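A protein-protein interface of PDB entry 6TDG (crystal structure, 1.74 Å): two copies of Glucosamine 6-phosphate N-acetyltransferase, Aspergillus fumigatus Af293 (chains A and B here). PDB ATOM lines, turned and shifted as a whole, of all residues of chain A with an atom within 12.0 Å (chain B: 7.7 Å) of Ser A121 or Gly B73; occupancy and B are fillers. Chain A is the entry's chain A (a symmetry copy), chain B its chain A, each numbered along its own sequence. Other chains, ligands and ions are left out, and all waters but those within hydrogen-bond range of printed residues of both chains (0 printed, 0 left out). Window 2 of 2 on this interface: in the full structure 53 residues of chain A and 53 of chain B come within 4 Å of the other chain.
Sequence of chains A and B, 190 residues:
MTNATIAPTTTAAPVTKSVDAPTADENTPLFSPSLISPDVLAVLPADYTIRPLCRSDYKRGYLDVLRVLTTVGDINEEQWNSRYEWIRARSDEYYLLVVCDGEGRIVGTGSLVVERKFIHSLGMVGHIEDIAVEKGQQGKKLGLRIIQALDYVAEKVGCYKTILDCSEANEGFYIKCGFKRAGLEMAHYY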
ATOM      1  N   VAL A 114      -8.506   0.947 -27.261  1.00  0.00           N
ATOM      2  CA  VAL A 114      -8.681   1.720 -26.013  1.00  0.00           C
ATOM      3  C   VAL A 114      -8.505   0.791 -24.835  1.00  0.00           C
ATOM      4  O   VAL A 114      -9.336  -0.092 -24.625  1.00  0.00           O
ATOM      5  CB  VAL A 114     -10.035   2.421 -25.993  1.00  0.00           C
ATOM      6  CG1 VAL A 114     -10.231   3.186 -24.691  1.00  0.00           C
ATOM      7  CG2 VAL A 114     -10.143   3.337 -27.192  1.00  0.00           C
ATOM      8  N   GLU A 115      -7.436   1.034 -24.087  1.00  0.00           N
ATOM      9  CA  GLU A 115      -7.016   0.240 -22.916  1.00  0.00           C
ATOM     10  C   GLU A 115      -7.644   0.875 -21.687  1.00  0.00           C
ATOM     11  O   GLU A 115      -7.555   2.092 -21.557  1.00  0.00           O
ATOM     12  CB  GLU A 115      -5.511   0.350 -22.734  1.00  0.00           C
ATOM     13  CG  GLU A 115      -4.961  -0.411 -21.539  1.00  0.00           C
ATOM     14  CD  GLU A 115      -3.558   0.011 -21.162  1.00  0.00           C
ATOM     15  OE1 GLU A 115      -3.027   0.921 -21.830  1.00  0.00           O
ATOM     16  OE2 GLU A 115      -3.036  -0.534 -20.159  1.00  0.00           O
ATOM     17  N   ARG A 116      -8.246   0.039 -20.849  1.00  0.00           N
ATOM     18  CA  ARG A 116      -8.767   0.455 -19.531  1.00  0.00           C
ATOM     19  C   ARG A 116      -7.683   0.240 -18.492  1.00  0.00           C
ATOM     20  O   ARG A 116      -7.018  -0.837 -18.504  1.00  0.00           O
ATOM     21  CB  ARG A 116     -10.022  -0.338 -19.177  1.00  0.00           C
ATOM     22  CG  ARG A 116     -11.287   0.299 -19.704  1.00  0.00           C
ATOM     23  CD  ARG A 116     -11.299   0.367 -21.206  1.00  0.00           C
ATOM     24  NE  ARG A 116     -12.646   0.710 -21.642  1.00  0.00           N
ATOM     25  CZ  ARG A 116     -13.048   0.722 -22.900  1.00  0.00           C
ATOM     26  NH1 ARG A 116     -12.224   0.316 -23.873  1.00  0.00           N
ATOM     27  NH2 ARG A 116     -14.301   1.077 -23.164  1.00  0.00           N
ATOM     28  N   LYS A 117      -7.561   1.222 -17.604  1.00  0.00           N
ATOM     29  CA  LYS A 117      -6.600   1.227 -16.483  1.00  0.00           C
ATOM     30  C   LYS A 117      -7.306   1.464 -15.127  1.00  0.00           C
ATOM     31  O   LYS A 117      -8.426   2.005 -15.093  1.00  0.00           O
ATOM     32  CB  LYS A 117      -5.549   2.296 -16.801  1.00  0.00           C
ATOM     33  CG  LYS A 117      -4.457   1.837 -17.768  1.00  0.00           C
ATOM     34  CD  LYS A 117      -3.327   2.806 -17.811  1.00  0.00           C
ATOM     35  CE  LYS A 117      -2.368   2.570 -18.944  1.00  0.00           C
ATOM     36  NZ  LYS A 117      -1.504   1.394 -18.705  1.00  0.00           N
ATOM     37  N   PHE A 118      -6.658   1.093 -14.013  1.00  0.00           N
ATOM     38  CA  PHE A 118      -7.076   1.563 -12.667  1.00  0.00           C
ATOM     39  C   PHE A 118      -6.484   2.969 -12.426  1.00  0.00           C
ATOM     40  O   PHE A 118      -7.181   3.824 -11.825  1.00  0.00           O
ATOM     41  CB  PHE A 118      -6.749   0.531 -11.580  1.00  0.00           C
ATOM     42  CG  PHE A 118      -7.676  -0.657 -11.565  1.00  0.00           C
ATOM     43  CD1 PHE A 118      -8.965  -0.552 -11.071  1.00  0.00           C
ATOM     44  CD2 PHE A 118      -7.256  -1.905 -12.007  1.00  0.00           C
ATOM     45  CE1 PHE A 118      -9.840  -1.642 -11.043  1.00  0.00           C
ATOM     46  CE2 PHE A 118      -8.119  -2.993 -11.998  1.00  0.00           C
ATOM     47  CZ  PHE A 118      -9.432  -2.865 -11.552  1.00  0.00           C
ATOM     48  N   ILE A 119      -5.240   3.226 -12.860  1.00  0.00           N
ATOM     49  CA  ILE A 119      -4.554   4.536 -12.654  1.00  0.00           C
ATOM     50  C   ILE A 119      -5.313   5.651 -13.379  1.00  0.00           C
ATOM     51  O   ILE A 119      -6.190   5.365 -14.253  1.00  0.00           O
ATOM     52  CB  ILE A 119      -3.073   4.499 -13.084  1.00  0.00           C
ATOM     53  CG1 ILE A 119      -2.887   4.221 -14.576  1.00  0.00           C
ATOM     54  CG2 ILE A 119      -2.325   3.481 -12.247  1.00  0.00           C
ATOM     55  CD1 ILE A 119      -1.462   4.449 -15.068  1.00  0.00           C
ATOM     56  N   HIS A 120      -4.955   6.888 -13.058  1.00  0.00           N
ATOM     57  CA  HIS A 120      -5.549   8.107 -13.685  1.00  0.00           C
ATOM     58  C   HIS A 120      -7.069   8.110 -13.526  1.00  0.00           C
ATOM     59  O   HIS A 120      -7.762   8.433 -14.510  1.00  0.00           O
ATOM     60  CB  HIS A 120      -5.147   8.144 -15.158  1.00  0.00           C
ATOM     61  CG  HIS A 120      -4.769   9.489 -15.661  1.00  0.00           C
ATOM     62  ND1 HIS A 120      -5.701  10.342 -16.254  1.00  0.00           N
ATOM     63  CD2 HIS A 120      -3.583  10.136 -15.652  1.00  0.00           C
ATOM     64  CE1 HIS A 120      -5.096  11.466 -16.596  1.00  0.00           C
ATOM     65  NE2 HIS A 120      -3.787  11.352 -16.250  1.00  0.00           N
ATOM     66  N   SER A 121      -7.569   7.763 -12.338  1.00  0.00           N
ATOM     67  CA  SER A 121      -9.015   7.704 -11.979  1.00  0.00           C
ATOM     68  C   SER A 121      -9.750   6.786 -12.963  1.00  0.00           C
ATOM     69  O   SER A 121     -10.771   7.216 -13.558  1.00  0.00           O
ATOM     70  CB  SER A 121      -9.681   9.072 -11.893  1.00  0.00           C
ATOM     71  OG  SER A 121      -8.972   9.940 -11.014  1.00  0.00           O
ATOM     72  N   LEU A 122      -9.307   5.530 -13.056  1.00  0.00           N
ATOM     73  CA  LEU A 122      -9.934   4.543 -13.964  1.00  0.00           C
ATOM     74  C   LEU A 122      -9.838   5.089 -15.397  1.00  0.00           C
ATOM     75  O   LEU A 122     -10.831   5.024 -16.149  1.00  0.00           O
ATOM     76  CB  LEU A 122     -11.386   4.328 -13.548  1.00  0.00           C
ATOM     77  CG  LEU A 122     -11.592   3.905 -12.089  1.00  0.00           C
ATOM     78  CD1 LEU A 122     -13.037   3.522 -11.849  1.00  0.00           C
ATOM     79  CD2 LEU A 122     -10.694   2.753 -11.698  1.00  0.00           C
ATOM     80  N   GLY A 123      -8.648   5.550 -15.764  1.00  0.00           N
ATOM     81  CA  GLY A 123      -8.406   6.201 -17.054  1.00  0.00           C
ATOM     82  C   GLY A 123      -8.392   5.198 -18.195  1.00  0.00           C
ATOM     83  O   GLY A 123      -8.474   3.979 -17.935  1.00  0.00           O
ATOM     84  N   MET A 124      -8.388   5.753 -19.397  1.00  0.00           N
ATOM     85  CA  MET A 124      -8.326   5.040 -20.688  1.00  0.00           C
ATOM     86  C   MET A 124      -7.203   5.642 -21.532  1.00  0.00           C
ATOM     87  O   MET A 124      -7.120   6.885 -21.690  1.00  0.00           O
ATOM     88  CB  MET A 124      -9.682   5.113 -21.404  1.00  0.00           C
ATOM     89  CG  MET A 124     -10.795   4.594 -20.510  1.00  0.00           C
ATOM     90  SD  MET A 124     -12.296   4.298 -21.410  1.00  0.00           S
ATOM     91  CE  MET A 124     -12.723   6.019 -21.681  1.00  0.00           C
ATOM     92  N   VAL A 125      -6.350   4.766 -22.065  1.00  0.00           N
ATOM     93  CA  VAL A 125      -5.258   5.156 -23.003  1.00  0.00           C
ATOM     94  C   VAL A 125      -5.614   4.656 -24.409  1.00  0.00           C
ATOM     95  O   VAL A 125      -5.974   3.480 -24.545  1.00  0.00           O
ATOM     96  CB  VAL A 125      -3.926   4.584 -22.518  1.00  0.00           C
ATOM     97  CG1 VAL A 125      -2.818   4.843 -23.529  1.00  0.00           C
ATOM     98  CG2 VAL A 125      -3.597   5.147 -21.140  1.00  0.00           C
ATOM     99  N   VAL A 157     -14.081   9.430 -26.986  1.00  0.00           N
ATOM    100  CA  VAL A 157     -14.464   8.351 -26.037  1.00  0.00           C
ATOM    101  C   VAL A 157     -13.794   8.551 -24.670  1.00  0.00           C
ATOM    102  O   VAL A 157     -14.007   7.670 -23.824  1.00  0.00           O
ATOM    103  CB  VAL A 157     -14.216   6.949 -26.655  1.00  0.00           C
ATOM    104  CG1 VAL A 157     -14.908   6.868 -27.999  1.00  0.00           C
ATOM    105  CG2 VAL A 157     -12.757   6.582 -26.853  1.00  0.00           C
ATOM    106  N   GLY A 158     -12.991   9.609 -24.453  1.00  0.00           N
ATOM    107  CA  GLY A 158     -12.463   9.946 -23.112  1.00  0.00           C
ATOM    108  C   GLY A 158     -11.058   9.405 -22.804  1.00  0.00           C
ATOM    109  O   GLY A 158     -10.699   9.353 -21.619  1.00  0.00           O
ATOM    110  N   CYS A 159     -10.224   9.070 -23.798  1.00  0.00           N
ATOM    111  CA  CYS A 159      -8.789   8.754 -23.524  1.00  0.00           C
ATOM    112  C   CYS A 159      -8.069   9.990 -22.949  1.00  0.00           C
ATOM    113  O   CYS A 159      -8.241  11.082 -23.506  1.00  0.00           O
ATOM    114  CB  CYS A 159      -8.101   8.271 -24.804  1.00  0.00           C
ATOM    115  SG  CYS A 159      -8.796   6.706 -25.330  1.00  0.00           S
ATOM    116  N   TYR A 160      -7.147   9.796 -22.002  1.00  0.00           N
ATOM    117  CA  TYR A 160      -6.330  10.901 -21.444  1.00  0.00           C
ATOM    118  C   TYR A 160      -5.108  11.130 -22.327  1.00  0.00           C
ATOM    119  O   TYR A 160      -4.553  12.235 -22.280  1.00  0.00           O
ATOM    120  CB  TYR A 160      -5.985  10.701 -19.964  1.00  0.00           C
ATOM    121  CG  TYR A 160      -5.068   9.567 -19.586  1.00  0.00           C
ATOM    122  CD1 TYR A 160      -3.694   9.729 -19.484  1.00  0.00           C
ATOM    123  CD2 TYR A 160      -5.615   8.359 -19.180  1.00  0.00           C
ATOM    124  CE1 TYR A 160      -2.882   8.692 -19.029  1.00  0.00           C
ATOM    125  CE2 TYR A 160      -4.824   7.312 -18.737  1.00  0.00           C
ATOM    126  CZ  TYR A 160      -3.455   7.475 -18.672  1.00  0.00           C
ATOM    127  OH  TYR A 160      -2.750   6.401 -18.209  1.00  0.00           O
ATOM    128  N   LYS A 161      -4.733  10.140 -23.150  1.00  0.00           N
ATOM    129  CA  LYS A 161      -3.654  10.310 -24.144  1.00  0.00           C
ATOM    130  C   LYS A 161      -3.823   9.224 -25.201  1.00  0.00           C
ATOM    131  O   LYS A 161      -4.512   8.224 -24.917  1.00  0.00           O
ATOM    132  CB  LYS A 161      -2.258  10.204 -23.516  1.00  0.00           C
ATOM    133  CG  LYS A 161      -1.915   8.855 -22.920  1.00  0.00           C
ATOM    134  CD  LYS A 161      -0.635   8.824 -22.159  1.00  0.00           C
ATOM    135  CE  LYS A 161      -0.319   7.437 -21.631  1.00  0.00           C
ATOM    136  NZ  LYS A 161       0.955   7.425 -20.871  1.00  0.00           N
ATOM    137  N   LEU B  63      -4.594  -0.640  -4.606  1.00  0.00           N
ATOM    138  CA  LEU B  63      -4.476   0.669  -5.297  1.00  0.00           C
ATOM    139  C   LEU B  63      -3.315   1.463  -4.710  1.00  0.00           C
ATOM    140  O   LEU B  63      -2.639   2.211  -5.456  1.00  0.00           O
ATOM    141  CB  LEU B  63      -5.799   1.421  -5.165  1.00  0.00           C
ATOM    142  CG  LEU B  63      -6.952   0.807  -5.944  1.00  0.00           C
ATOM    143  CD1 LEU B  63      -8.246   1.510  -5.591  1.00  0.00           C
ATOM    144  CD2 LEU B  63      -6.695   0.878  -7.458  1.00  0.00           C
ATOM    145  N   ARG B  67       0.144   3.571  -6.613  1.00  0.00           N
ATOM    146  CA  ARG B  67       0.596   4.967  -6.359  1.00  0.00           C
ATOM    147  C   ARG B  67       2.093   5.126  -6.627  1.00  0.00           C
ATOM    148  O   ARG B  67       2.510   6.261  -6.891  1.00  0.00           O
ATOM    149  CB  ARG B  67       0.199   5.387  -4.941  1.00  0.00           C
ATOM    150  CG  ARG B  67      -1.311   5.338  -4.751  1.00  0.00           C
ATOM    151  CD  ARG B  67      -1.814   5.973  -3.474  1.00  0.00           C
ATOM    152  NE  ARG B  67      -3.133   5.422  -3.189  1.00  0.00           N
ATOM    153  CZ  ARG B  67      -4.261   5.769  -3.800  1.00  0.00           C
ATOM    154  NH1 ARG B  67      -4.266   6.712  -4.729  1.00  0.00           N
ATOM    155  NH2 ARG B  67      -5.392   5.174  -3.461  1.00  0.00           N
ATOM    156  N   THR B  70       2.210   6.384 -10.681  1.00  0.00           N
ATOM    157  CA  THR B  70       1.635   7.688 -11.043  1.00  0.00           C
ATOM    158  C   THR B  70       0.375   7.855 -10.199  1.00  0.00           C
ATOM    159  O   THR B  70       0.043   6.931  -9.389  1.00  0.00           O
ATOM    160  CB  THR B  70       1.362   7.745 -12.554  1.00  0.00           C
ATOM    161  OG1 THR B  70       0.853   9.041 -12.876  1.00  0.00           O
ATOM    162  CG2 THR B  70       0.402   6.664 -13.005  1.00  0.00           C
ATOM    163  N   THR B  71      -0.286   8.989 -10.394  1.00  0.00           N
ATOM    164  CA  THR B  71      -1.565   9.327  -9.743  1.00  0.00           C
ATOM    165  C   THR B  71      -2.553   8.209 -10.045  1.00  0.00           C
ATOM    166  O   THR B  71      -2.742   7.858 -11.229  1.00  0.00           O
ATOM    167  CB  THR B  71      -2.109  10.675 -10.228  1.00  0.00           C
ATOM    168  OG1 THR B  71      -1.353  11.665  -9.530  1.00  0.00           O
ATOM    169  CG2 THR B  71      -3.592  10.851  -9.971  1.00  0.00           C
ATOM    170  N   VAL B  72      -3.201   7.714  -9.004  1.00  0.00           N
ATOM    171  CA  VAL B  72      -4.282   6.707  -9.154  1.00  0.00           C
ATOM    172  C   VAL B  72      -5.625   7.431  -9.128  1.00  0.00           C
ATOM    173  O   VAL B  72      -6.519   7.003  -9.881  1.00  0.00           O
ATOM    174  CB  VAL B  72      -4.163   5.635  -8.053  1.00  0.00           C
ATOM    175  CG1 VAL B  72      -5.335   4.673  -8.100  1.00  0.00           C
ATOM    176  CG2 VAL B  72      -2.828   4.910  -8.146  1.00  0.00           C
ATOM    177  N   GLY B  73      -5.729   8.492  -8.309  1.00  0.00           N
ATOM    178  CA  GLY B  73      -6.993   9.189  -7.964  1.00  0.00           C
ATOM    179  C   GLY B  73      -7.616   8.585  -6.710  1.00  0.00           C
ATOM    180  O   GLY B  73      -6.962   7.740  -6.070  1.00  0.00           O
ATOM    181  N   ASP B  74      -8.817   9.022  -6.327  1.00  0.00           N
ATOM    182  CA  ASP B  74      -9.633   8.381  -5.256  1.00  0.00           C
ATOM    183  C   ASP B  74     -10.672   7.496  -5.942  1.00  0.00           C
ATOM    184  O   ASP B  74     -11.511   8.031  -6.682  1.00  0.00           O
ATOM    185  CB  ASP B  74     -10.347   9.387  -4.345  1.00  0.00           C
ATOM    186  CG  ASP B  74      -9.476   9.990  -3.253  1.00  0.00           C
ATOM    187  OD1 ASP B  74      -8.874   9.202  -2.471  1.00  0.00           O
ATOM    188  OD2 ASP B  74      -9.406  11.244  -3.190  1.00  0.00           O
ATOM    189  N   ILE B  75     -10.592   6.184  -5.726  1.00  0.00           N
ATOM    190  CA  ILE B  75     -11.552   5.183  -6.263  1.00  0.00           C
ATOM    191  C   ILE B  75     -12.233   4.532  -5.053  1.00  0.00           C
ATOM    192  O   ILE B  75     -11.526   3.914  -4.222  1.00  0.00           O
ATOM    193  CB  ILE B  75     -10.790   4.174  -7.152  1.00  0.00           C
ATOM    194  CG1 ILE B  75     -10.079   4.871  -8.318  1.00  0.00           C
ATOM    195  CG2 ILE B  75     -11.691   3.054  -7.636  1.00  0.00           C
ATOM    196  CD1 ILE B  75      -9.011   4.029  -8.966  1.00  0.00           C
ATOM    197  N   ASN B  76     -13.555   4.613  -4.961  1.00  0.00           N
ATOM    198  CA  ASN B  76     -14.320   3.923  -3.881  1.00  0.00           C
ATOM    199  C   ASN B  76     -14.602   2.475  -4.302  1.00  0.00           C
ATOM    200  O   ASN B  76     -14.266   2.094  -5.448  1.00  0.00           O
ATOM    201  CB  ASN B  76     -15.570   4.710  -3.457  1.00  0.00           C
ATOM    202  CG  ASN B  76     -16.730   4.605  -4.413  1.00  0.00           C
ATOM    203  OD1 ASN B  76     -16.683   3.849  -5.382  1.00  0.00           O
ATOM    204  ND2 ASN B  76     -17.797   5.347  -4.130  1.00  0.00           N
ATOM    205  N   GLN B  79     -16.911   1.740  -7.417  1.00  0.00           N
ATOM    206  CA  GLN B  79     -16.248   2.072  -8.714  1.00  0.00           C
ATOM    207  C   GLN B  79     -15.276   0.918  -9.028  1.00  0.00           C
ATOM    208  O   GLN B  79     -15.265   0.445 -10.135  1.00  0.00           O
ATOM    209  CB  GLN B  79     -15.479   3.374  -8.623  1.00  0.00           C
ATOM    210  CG  GLN B  79     -16.320   4.635  -8.827  1.00  0.00           C
ATOM    211  CD  GLN B  79     -15.444   5.842  -8.593  1.00  0.00           C
ATOM    212  OE1 GLN B  79     -14.886   6.014  -7.507  1.00  0.00           O
ATOM    213  NE2 GLN B  79     -15.287   6.677  -9.610  1.00  0.00           N
ATOM    214  N   ARG B  83     -15.325  -1.507 -12.385  1.00  0.00           N
ATOM    215  CA  ARG B  83     -14.205  -1.712 -13.326  1.00  0.00           C
ATOM    216  C   ARG B  83     -13.786  -3.187 -13.267  1.00  0.00           C
ATOM    217  O   ARG B  83     -13.550  -3.760 -14.338  1.00  0.00           O
ATOM    218  CB  ARG B  83     -13.029  -0.793 -13.001  1.00  0.00           C
ATOM    219  CG  ARG B  83     -11.908  -0.895 -14.022  1.00  0.00           C
ATOM    220  CD  ARG B  83     -12.350  -0.337 -15.374  1.00  0.00           C
ATOM    221  NE  ARG B  83     -11.342   0.626 -15.803  1.00  0.00           N
ATOM    222  CZ  ARG B  83     -11.575   1.800 -16.368  1.00  0.00           C
ATOM    223  NH1 ARG B  83     -12.801   2.201 -16.604  1.00  0.00           N
ATOM    224  NH2 ARG B  83     -10.562   2.570 -16.694  1.00  0.00           N
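The guanidinium group (NH1) of Arg B67 lies within hydrogen-bond range of the backbone carbonyl oxygen (O) of Gly B73 (3.2 Å). NH1 of Arg A116 sits at hydrogen-bond distance from O of Val A114 (3.0 Å). The side-chain carboxylate of Glu A115 is in salt-bridge range of the side-chain amino group of Lys A117 (2.9 Å). The guanidinium group (NE) of Arg A116 sits at hydrogen-bond distance from the side-chain sulfur (SD) of Met A124, 3.6 Å away. The backbone NH of Lys A117 sits at hydrogen-bond distance from the backbone carbonyl oxygen of Gly A123.
Ser A121 touches just these residues of chain B: Val B72 (2.8 Å) and Gly B73 (3.7 Å). Of chain A, only Ser A121 comes within 4 Å of Gly B73. Of chain A, only Phe A118 (3.8 Å), Ile A119 (3.9 Å), His A120 (3.5 Å) and Ser A121 (2.8 Å) come within 4 Å of Val B72. No residue of chain A comes within 4 Å of Asp B74. Of the printed residues of chain B, Arg A116 touches Arg B83 (3.7 Å). Of the printed residues of chain A, Thr B70 touches Ile A119. Printed residues of chain A within 4 Å of Arg B83: Arg A116, Lys A117, Phe A118, Leu A122 and Gly A123. The nearest printed residue of chain B that does not touch Ser A121 is Ile B75 (4.7 Å).
No position is printed for both chains.
Arg A116 touches Arg B83 (CG to CZ, 3.7 Å). Phe A118 touches Val B72 (O to O, 3.8 Å). O of Phe A118 touches CD1 of Ile B75 (3.4 Å). CG of Arg B83 touches CE1 of Phe A118 (3.7 Å). Thr B70 touches Ile A119 (CG2 to CD1, 3.6 Å). Thr B71 touches Ile A119. C of Ile A119 touches O of Val B72, at 3.9 Å. Val B72 touches His A120. OG of Ser A121 touches CA of Gly B73 (3.7 Å). Leu A122 touches Ile B75 (CD2 to CD1, 3.5 Å).
The backbone NH (N) of His A120 sits at hydrogen-bond distance from the backbone carbonyl oxygen (O) of Thr B71 (3.0 Å). O of Val B72 sits at hydrogen-bond distance from N of Ser A121, 2.8 Å away. The guanidinium group (NH2) of Arg B83 is in hydrogen-bond range of the backbone carbonyl oxygen (O) of Lys A117. The guanidinium group of Arg B83 sits at hydrogen-bond distance from the backbone carbonyl oxygen of Leu A122 (2.5 Å). O of Gly A123 is in hydrogen-bond range of NH2 of Arg B83, at 2.8 Å.
Hydrophobic or aromatic side chains of chain B that line the printed part of chain A: Ile B75. Of the 17 printed residues of chain A, 8 touch a printed residue of chain B. Hydrophobic or aromatic side chains of chain A that line the printed part of chain B: Phe A118, Ile A119 and Leu A122.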
